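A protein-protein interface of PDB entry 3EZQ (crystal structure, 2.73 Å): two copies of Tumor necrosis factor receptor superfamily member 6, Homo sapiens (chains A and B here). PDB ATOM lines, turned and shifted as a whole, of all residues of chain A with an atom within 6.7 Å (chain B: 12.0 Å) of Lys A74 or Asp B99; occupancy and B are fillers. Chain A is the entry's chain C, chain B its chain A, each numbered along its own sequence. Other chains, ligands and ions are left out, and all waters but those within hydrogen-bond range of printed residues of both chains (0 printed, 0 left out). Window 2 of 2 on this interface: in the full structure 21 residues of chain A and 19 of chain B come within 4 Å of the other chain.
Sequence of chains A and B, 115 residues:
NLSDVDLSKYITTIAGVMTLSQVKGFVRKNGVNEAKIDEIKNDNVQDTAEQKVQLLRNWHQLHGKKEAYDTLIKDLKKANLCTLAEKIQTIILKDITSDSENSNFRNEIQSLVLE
NZ of Lys A74 lies within salt-bridge range of OD1 of Asp B99 (3.1 Å). O of Asp B95 lies close to NZ of Lys A77, at 3.4 Å. NZ of Lys A77 lies close to O of Ser B100 (2.3 Å).
The side-chain carboxylate (OD1) of Asp B95 sits at hydrogen-bond distance from the side-chain amide nitrogen (ND2) of Asn B102, at 2.4 Å. The side-chain hydroxyl of Ser B98 lies within hydrogen-bond range of the backbone NH of Ser B100 (3.0 Å). The side-chain amide oxygen of Asn B104 lies close to the side-chain amide oxygen of Asn B102, at 2.9 Å.
OE2 of Glu B101 touches CG2 of Ile A73, at 3.2 Å. O of Ser B98 touches NZ of Lys A77 (3.6 Å). Asn B102 touches Lys A77 (ND2 to NZ, 3.8 Å). Lys A78 touches Ile B96.
No residue of chain B comes within 4 Å of Asp A70. No residue of chain B comes within 4 Å of Thr A71. Lys A74 touches just one residue of chain B: Asp B99. No residue of chain B comes within 4 Å of Leu A76. Printed residues of chain B within 4 Å of Lys A78: Ile B96. Leu B93 touches none of the printed residues of chain A. Lys B94 touches none of the printed residues of chain A. Of chain A, only Lys A74 comes within 4 Å of Asp B99. Printed residues of chain A within 4 Å of Ser B100: Lys A77. Of the printed residues of chain A, Asn B102 touches Lys A77 (3.8 Å). The nearest residue of chain A that does not touch Asp B99 is Lys A77 (4.5 Å).
Of the 12 printed residues of chain A, 4 touch a printed residue of chain B. Printed residues of chain A that touch a printed residue of chain B: Ile A73, Lys A74, Lys A77 and Lys A78. Printed residues of chain B that touch a printed residue of chain A: Asp B95, Ile B96, Ser B98, Asp B99, Ser B100, Glu B101 and Asn B102. Among the printed residues, Asp or Glu carboxylates within 4 Å of a Lys or Arg side-chain nitrogen of the other chain: Lys A74 with Asp B99.
No position is printed for both chains. Of the 7 pairs that touch across the chains among the printed residues, none has its exchanged pair printed and touching as well.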
ATOM      1  N   PHE A  26      -5.947  -9.325  33.558  1.00  0.00           N
ATOM      2  CA  PHE A  26      -6.334 -10.649  34.013  1.00  0.00           C
ATOM      3  C   PHE A  26      -7.116 -10.627  35.313  1.00  0.00           C
ATOM      4  O   PHE A  26      -8.243 -11.140  35.369  1.00  0.00           O
ATOM      5  CB  PHE A  26      -5.086 -11.499  34.182  1.00  0.00           C
ATOM      6  CG  PHE A  26      -5.354 -12.845  34.730  1.00  0.00           C
ATOM      7  CD1 PHE A  26      -6.030 -13.779  33.984  1.00  0.00           C
ATOM      8  CD2 PHE A  26      -4.920 -13.191  35.981  1.00  0.00           C
ATOM      9  CE1 PHE A  26      -6.275 -15.031  34.474  1.00  0.00           C
ATOM     10  CE2 PHE A  26      -5.167 -14.443  36.469  1.00  0.00           C
ATOM     11  CZ  PHE A  26      -5.851 -15.362  35.707  1.00  0.00           C
ATOM     12  N   TYR A  69      -6.842 -22.439  37.852  1.00  0.00           N
ATOM     13  CA  TYR A  69      -6.080 -23.093  36.785  1.00  0.00           C
ATOM     14  C   TYR A  69      -6.582 -22.690  35.425  1.00  0.00           C
ATOM     15  O   TYR A  69      -5.855 -22.095  34.639  1.00  0.00           O
ATOM     16  CB  TYR A  69      -6.210 -24.609  36.862  1.00  0.00           C
ATOM     17  CG  TYR A  69      -5.208 -25.286  37.750  1.00  0.00           C
ATOM     18  CD1 TYR A  69      -3.851 -25.228  37.462  1.00  0.00           C
ATOM     19  CD2 TYR A  69      -5.621 -26.031  38.861  1.00  0.00           C
ATOM     20  CE1 TYR A  69      -2.933 -25.875  38.269  1.00  0.00           C
ATOM     21  CE2 TYR A  69      -4.714 -26.676  39.663  1.00  0.00           C
ATOM     22  CZ  TYR A  69      -3.373 -26.597  39.364  1.00  0.00           C
ATOM     23  OH  TYR A  69      -2.468 -27.244  40.158  1.00  0.00           O
ATOM     24  N   ASP A  70      -7.835 -23.044  35.146  1.00  0.00           N
ATOM     25  CA  ASP A  70      -8.403 -22.852  33.810  1.00  0.00           C
ATOM     26  C   ASP A  70      -8.185 -21.417  33.359  1.00  0.00           C
ATOM     27  O   ASP A  70      -7.661 -21.195  32.290  1.00  0.00           O
ATOM     28  CB  ASP A  70      -9.901 -23.213  33.764  1.00  0.00           C
ATOM     29  CG  ASP A  70     -10.155 -24.729  33.781  1.00  0.00           C
ATOM     30  OD1 ASP A  70      -9.141 -25.504  33.777  1.00  0.00           O
ATOM     31  OD2 ASP A  70     -11.373 -25.151  33.802  1.00  0.00           O
ATOM     32  N   THR A  71      -8.528 -20.450  34.204  1.00  0.00           N
ATOM     33  CA  THR A  71      -8.411 -19.042  33.828  1.00  0.00           C
ATOM     34  C   THR A  71      -6.955 -18.618  33.576  1.00  0.00           C
ATOM     35  O   THR A  71      -6.678 -18.002  32.550  1.00  0.00           O
ATOM     36  CB  THR A  71      -9.049 -18.096  34.849  1.00  0.00           C
ATOM     37  OG1 THR A  71      -8.745 -18.554  36.161  1.00  0.00           O
ATOM     38  CG2 THR A  71     -10.550 -18.052  34.660  1.00  0.00           C
ATOM     39  N   LEU A  72      -6.039 -18.948  34.491  1.00  0.00           N
ATOM     40  CA  LEU A  72      -4.626 -18.572  34.347  1.00  0.00           C
ATOM     41  C   LEU A  72      -3.970 -19.232  33.151  1.00  0.00           C
ATOM     42  O   LEU A  72      -3.271 -18.545  32.397  1.00  0.00           O
ATOM     43  CB  LEU A  72      -3.813 -18.877  35.617  1.00  0.00           C
ATOM     44  CG  LEU A  72      -2.306 -18.517  35.596  1.00  0.00           C
ATOM     45  CD1 LEU A  72      -2.044 -17.034  35.465  1.00  0.00           C
ATOM     46  CD2 LEU A  72      -1.553 -19.032  36.811  1.00  0.00           C
ATOM     47  N   ILE A  73      -4.189 -20.541  32.976  1.00  0.00           N
ATOM     48  CA  ILE A  73      -3.650 -21.294  31.829  1.00  0.00           C
ATOM     49  C   ILE A  73      -4.139 -20.667  30.515  1.00  0.00           C
ATOM     50  O   ILE A  73      -3.337 -20.374  29.629  1.00  0.00           O
ATOM     51  CB  ILE A  73      -4.008 -22.819  31.917  1.00  0.00           C
ATOM     52  CG1 ILE A  73      -3.168 -23.513  32.993  1.00  0.00           C
ATOM     53  CG2 ILE A  73      -3.813 -23.545  30.574  1.00  0.00           C
ATOM     54  CD1 ILE A  73      -3.888 -24.705  33.650  1.00  0.00           C
ATOM     55  N   LYS A  74      -5.449 -20.448  30.419  1.00  0.00           N
ATOM     56  CA  LYS A  74      -6.067 -19.844  29.248  1.00  0.00           C
ATOM     57  C   LYS A  74      -5.442 -18.494  28.977  1.00  0.00           C
ATOM     58  O   LYS A  74      -5.153 -18.165  27.829  1.00  0.00           O
ATOM     59  CB  LYS A  74      -7.568 -19.697  29.485  1.00  0.00           C
ATOM     60  CG  LYS A  74      -8.342 -19.106  28.319  1.00  0.00           C
ATOM     61  CD  LYS A  74      -9.844 -19.406  28.471  1.00  0.00           C
ATOM     62  CE  LYS A  74     -10.285 -20.539  27.530  1.00  0.00           C
ATOM     63  NZ  LYS A  74     -11.694 -20.993  27.819  1.00  0.00           N
ATOM     64  N   ASP A  75      -5.204 -17.728  30.030  1.00  0.00           N
ATOM     65  CA  ASP A  75      -4.644 -16.394  29.859  1.00  0.00           C
ATOM     66  C   ASP A  75      -3.215 -16.435  29.331  1.00  0.00           C
ATOM     67  O   ASP A  75      -2.869 -15.681  28.413  1.00  0.00           O
ATOM     68  CB  ASP A  75      -4.681 -15.607  31.162  1.00  0.00           C
ATOM     69  CG  ASP A  75      -3.928 -14.309  31.063  1.00  0.00           C
ATOM     70  OD1 ASP A  75      -2.681 -14.365  31.031  1.00  0.00           O
ATOM     71  OD2 ASP A  75      -4.586 -13.251  31.008  1.00  0.00           O
ATOM     72  N   LEU A  76      -2.393 -17.309  29.912  1.00  0.00           N
ATOM     73  CA  LEU A  76      -1.025 -17.472  29.435  1.00  0.00           C
ATOM     74  C   LEU A  76      -0.966 -18.046  28.005  1.00  0.00           C
ATOM     75  O   LEU A  76      -0.094 -17.660  27.228  1.00  0.00           O
ATOM     76  CB  LEU A  76      -0.204 -18.343  30.389  1.00  0.00           C
ATOM     77  CG  LEU A  76       0.000 -17.810  31.806  1.00  0.00           C
ATOM     78  CD1 LEU A  76       0.869 -18.758  32.631  1.00  0.00           C
ATOM     79  CD2 LEU A  76       0.582 -16.388  31.808  1.00  0.00           C
ATOM     80  N   LYS A  77      -1.887 -18.954  27.670  1.00  0.00           N
ATOM     81  CA  LYS A  77      -1.928 -19.565  26.347  1.00  0.00           C
ATOM     82  C   LYS A  77      -2.149 -18.482  25.306  1.00  0.00           C
ATOM     83  O   LYS A  77      -1.383 -18.372  24.335  1.00  0.00           O
ATOM     84  CB  LYS A  77      -3.018 -20.636  26.263  1.00  0.00           C
ATOM     85  CG  LYS A  77      -2.869 -21.624  25.093  1.00  0.00           C
ATOM     86  CD  LYS A  77      -3.965 -22.699  25.110  1.00  0.00           C
ATOM     87  CE  LYS A  77      -4.945 -22.585  23.941  1.00  0.00           C
ATOM     88  NZ  LYS A  77      -6.035 -23.595  23.998  1.00  0.00           N
ATOM     89  N   LYS A  78      -3.168 -17.658  25.514  1.00  0.00           N
ATOM     90  CA  LYS A  78      -3.457 -16.618  24.542  1.00  0.00           C
ATOM     91  C   LYS A  78      -2.304 -15.626  24.436  1.00  0.00           C
ATOM     92  O   LYS A  78      -1.915 -15.225  23.351  1.00  0.00           O
ATOM     93  CB  LYS A  78      -4.769 -15.923  24.860  1.00  0.00           C
ATOM     94  CG  LYS A  78      -5.936 -16.862  24.744  1.00  0.00           C
ATOM     95  CD  LYS A  78      -7.228 -16.210  25.169  1.00  0.00           C
ATOM     96  CE  LYS A  78      -8.421 -17.082  24.812  1.00  0.00           C
ATOM     97  NZ  LYS A  78      -9.703 -16.336  25.023  1.00  0.00           N
ATOM     98  N   ALA A  79      -1.725 -15.229  25.546  1.00  0.00           N
ATOM     99  CA  ALA A  79      -0.631 -14.262  25.475  1.00  0.00           C
ATOM    100  C   ALA A  79       0.557 -14.887  24.733  1.00  0.00           C
ATOM    101  O   ALA A  79       1.162 -14.260  23.874  1.00  0.00           O
ATOM    102  CB  ALA A  79      -0.228 -13.815  26.828  1.00  0.00           C
ATOM    103  N   ILE B  91      -2.448 -22.935  12.697  1.00  0.00           N
ATOM    104  CA  ILE B  91      -2.238 -23.495  14.037  1.00  0.00           C
ATOM    105  C   ILE B  91      -2.551 -22.457  15.121  1.00  0.00           C
ATOM    106  O   ILE B  91      -3.327 -22.718  16.019  1.00  0.00           O
ATOM    107  CB  ILE B  91      -0.776 -23.998  14.168  1.00  0.00           C
ATOM    108  CG1 ILE B  91      -0.588 -25.290  13.346  1.00  0.00           C
ATOM    109  CG2 ILE B  91      -0.395 -24.191  15.655  1.00  0.00           C
ATOM    110  CD1 ILE B  91       0.791 -25.407  12.666  1.00  0.00           C
ATOM    111  N   ILE B  92      -1.980 -21.275  14.981  1.00  0.00           N
ATOM    112  CA  ILE B  92      -2.157 -20.200  15.950  1.00  0.00           C
ATOM    113  C   ILE B  92      -3.620 -19.799  16.119  1.00  0.00           C
ATOM    114  O   ILE B  92      -4.108 -19.775  17.251  1.00  0.00           O
ATOM    115  CB  ILE B  92      -1.302 -18.968  15.609  1.00  0.00           C
ATOM    116  CG1 ILE B  92       0.179 -19.357  15.750  1.00  0.00           C
ATOM    117  CG2 ILE B  92      -1.704 -17.833  16.513  1.00  0.00           C
ATOM    118  CD1 ILE B  92       1.173 -18.295  15.499  1.00  0.00           C
ATOM    119  N   LEU B  93      -4.330 -19.522  15.022  1.00  0.00           N
ATOM    120  CA  LEU B  93      -5.759 -19.167  15.133  1.00  0.00           C
ATOM    121  C   LEU B  93      -6.575 -20.292  15.735  1.00  0.00           C
ATOM    122  O   LEU B  93      -7.511 -20.070  16.506  1.00  0.00           O
ATOM    123  CB  LEU B  93      -6.359 -18.802  13.786  1.00  0.00           C
ATOM    124  CG  LEU B  93      -5.669 -17.571  13.175  1.00  0.00           C
ATOM    125  CD1 LEU B  93      -5.950 -17.449  11.661  1.00  0.00           C
ATOM    126  CD2 LEU B  93      -6.078 -16.341  13.983  1.00  0.00           C
ATOM    127  N   LYS B  94      -6.243 -21.517  15.378  1.00  0.00           N
ATOM    128  CA  LYS B  94      -6.934 -22.662  15.928  1.00  0.00           C
ATOM    129  C   LYS B  94      -6.736 -22.680  17.442  1.00  0.00           C
ATOM    130  O   LYS B  94      -7.696 -22.663  18.190  1.00  0.00           O
ATOM    131  CB  LYS B  94      -6.406 -23.924  15.234  1.00  0.00           C
ATOM    132  CG  LYS B  94      -6.754 -25.258  15.886  1.00  0.00           C
ATOM    133  CD  LYS B  94      -5.908 -26.395  15.282  1.00  0.00           C
ATOM    134  CE  LYS B  94      -5.702 -27.574  16.267  1.00  0.00           C
ATOM    135  NZ  LYS B  94      -6.949 -28.159  16.876  1.00  0.00           N
ATOM    136  N   ASP B  95      -5.493 -22.624  17.902  1.00  0.00           N
ATOM    137  CA  ASP B  95      -5.226 -22.666  19.347  1.00  0.00           C
ATOM    138  C   ASP B  95      -5.656 -21.434  20.143  1.00  0.00           C
ATOM    139  O   ASP B  95      -6.006 -21.562  21.289  1.00  0.00           O
ATOM    140  CB  ASP B  95      -3.756 -22.973  19.605  1.00  0.00           C
ATOM    141  CG  ASP B  95      -3.315 -24.262  18.947  1.00  0.00           C
ATOM    142  OD1 ASP B  95      -4.185 -25.136  18.674  1.00  0.00           O
ATOM    143  OD2 ASP B  95      -2.096 -24.395  18.672  1.00  0.00           O
ATOM    144  N   ILE B  96      -5.650 -20.260  19.528  1.00  0.00           N
ATOM    145  CA  ILE B  96      -5.960 -19.025  20.231  1.00  0.00           C
ATOM    146  C   ILE B  96      -7.459 -18.908  20.434  1.00  0.00           C
ATOM    147  O   ILE B  96      -7.904 -18.100  21.211  1.00  0.00           O
ATOM    148  CB  ILE B  96      -5.467 -17.785  19.453  1.00  0.00           C
ATOM    149  CG1 ILE B  96      -5.122 -16.663  20.408  1.00  0.00           C
ATOM    150  CG2 ILE B  96      -6.528 -17.323  18.446  1.00  0.00           C
ATOM    151  CD1 ILE B  96      -3.995 -15.772  19.859  1.00  0.00           C
ATOM    152  N   THR B  97      -8.237 -19.700  19.716  1.00  0.00           N
ATOM    153  CA  THR B  97      -9.701 -19.600  19.764  1.00  0.00           C
ATOM    154  C   THR B  97     -10.310 -20.850  20.400  1.00  0.00           C
ATOM    155  O   THR B  97     -11.528 -20.942  20.571  1.00  0.00           O
ATOM    156  CB  THR B  97     -10.345 -19.414  18.377  1.00  0.00           C
ATOM    157  OG1 THR B  97      -9.944 -20.473  17.521  1.00  0.00           O
ATOM    158  CG2 THR B  97      -9.919 -18.111  17.762  1.00  0.00           C
ATOM    159  N   SER B  98      -9.452 -21.787  20.783  1.00  0.00           N
ATOM    160  CA  SER B  98      -9.860 -22.985  21.500  1.00  0.00           C
ATOM    161  C   SER B  98      -9.923 -22.744  23.004  1.00  0.00           C
ATOM    162  O   SER B  98      -9.204 -21.916  23.545  1.00  0.00           O
ATOM    163  CB  SER B  98      -8.874 -24.106  21.206  1.00  0.00           C
ATOM    164  OG  SER B  98      -8.943 -25.094  22.206  1.00  0.00           O
ATOM    165  N   ASP B  99     -10.782 -23.497  23.668  1.00  0.00           N
ATOM    166  CA  ASP B  99     -10.905 -23.465  25.120  1.00  0.00           C
ATOM    167  C   ASP B  99     -10.088 -24.573  25.800  1.00  0.00           C
ATOM    168  O   ASP B  99      -9.767 -24.499  26.988  1.00  0.00           O
ATOM    169  CB  ASP B  99     -12.390 -23.629  25.488  1.00  0.00           C
ATOM    170  CG  ASP B  99     -13.240 -22.447  25.016  1.00  0.00           C
ATOM    171  OD1 ASP B  99     -13.955 -21.862  25.860  1.00  0.00           O
ATOM    172  OD2 ASP B  99     -13.180 -22.083  23.820  1.00  0.00           O
ATOM    173  N   SER B 100      -9.752 -25.604  25.048  1.00  0.00           N
ATOM    174  CA  SER B 100      -8.978 -26.699  25.610  1.00  0.00           C
ATOM    175  C   SER B 100      -7.511 -26.347  25.600  1.00  0.00           C
ATOM    176  O   SER B 100      -7.121 -25.321  25.047  1.00  0.00           O
ATOM    177  CB  SER B 100      -9.259 -28.038  24.886  1.00  0.00           C
ATOM    178  OG  SER B 100     -10.131 -28.888  25.665  1.00  0.00           O
ATOM    179  N   GLU B 101      -6.712 -27.168  26.268  1.00  0.00           N
ATOM    180  CA  GLU B 101      -5.263 -27.101  26.170  1.00  0.00           C
ATOM    181  C   GLU B 101      -4.792 -27.426  24.771  1.00  0.00           C
ATOM    182  O   GLU B 101      -5.403 -28.270  24.120  1.00  0.00           O
ATOM    183  CB  GLU B 101      -4.611 -28.152  27.059  1.00  0.00           C
ATOM    184  CG  GLU B 101      -3.192 -27.804  27.342  1.00  0.00           C
ATOM    185  CD  GLU B 101      -3.129 -26.439  27.984  1.00  0.00           C
ATOM    186  OE1 GLU B 101      -2.137 -25.704  27.759  1.00  0.00           O
ATOM    187  OE2 GLU B 101      -4.111 -26.098  28.691  1.00  0.00           O
ATOM    188  N   ASN B 102      -3.699 -26.803  24.322  1.00  0.00           N
ATOM    189  CA  ASN B 102      -3.049 -27.255  23.082  1.00  0.00           C
ATOM    190  C   ASN B 102      -1.568 -27.557  23.304  1.00  0.00           C
ATOM    191  O   ASN B 102      -0.675 -26.939  22.730  1.00  0.00           O
ATOM    192  CB  ASN B 102      -3.216 -26.210  21.979  1.00  0.00           C
ATOM    193  CG  ASN B 102      -4.375 -26.522  21.051  1.00  0.00           C
ATOM    194  OD1 ASN B 102      -4.506 -27.643  20.563  1.00  0.00           O
ATOM    195  ND2 ASN B 102      -5.219 -25.528  20.807  1.00  0.00           N
ATOM    196  N   SER B 103      -1.331 -28.562  24.142  1.00  0.00           N
ATOM    197  CA  SER B 103       0.026 -29.084  24.391  1.00  0.00           C
ATOM    198  C   SER B 103       0.739 -29.550  23.104  1.00  0.00           C
ATOM    199  O   SER B 103       1.917 -29.935  23.144  1.00  0.00           O
ATOM    200  CB  SER B 103      -0.010 -30.243  25.403  1.00  0.00           C
ATOM    201  OG  SER B 103       1.231 -30.938  25.433  1.00  0.00           O
ATOM    202  N   ASN B 104       0.028 -29.522  21.977  1.00  0.00           N
ATOM    203  CA  ASN B 104       0.579 -29.954  20.691  1.00  0.00           C
ATOM    204  C   ASN B 104       1.246 -28.810  19.887  1.00  0.00           C
ATOM    205  O   ASN B 104       1.925 -29.060  18.872  1.00  0.00           O
ATOM    206  CB  ASN B 104      -0.510 -30.677  19.850  1.00  0.00           C
ATOM    207  CG  ASN B 104      -1.884 -29.943  19.854  1.00  0.00           C
ATOM    208  OD1 ASN B 104      -1.951 -28.725  19.630  1.00  0.00           O
ATOM    209  ND2 ASN B 104      -2.973 -30.690  20.096  1.00  0.00           N
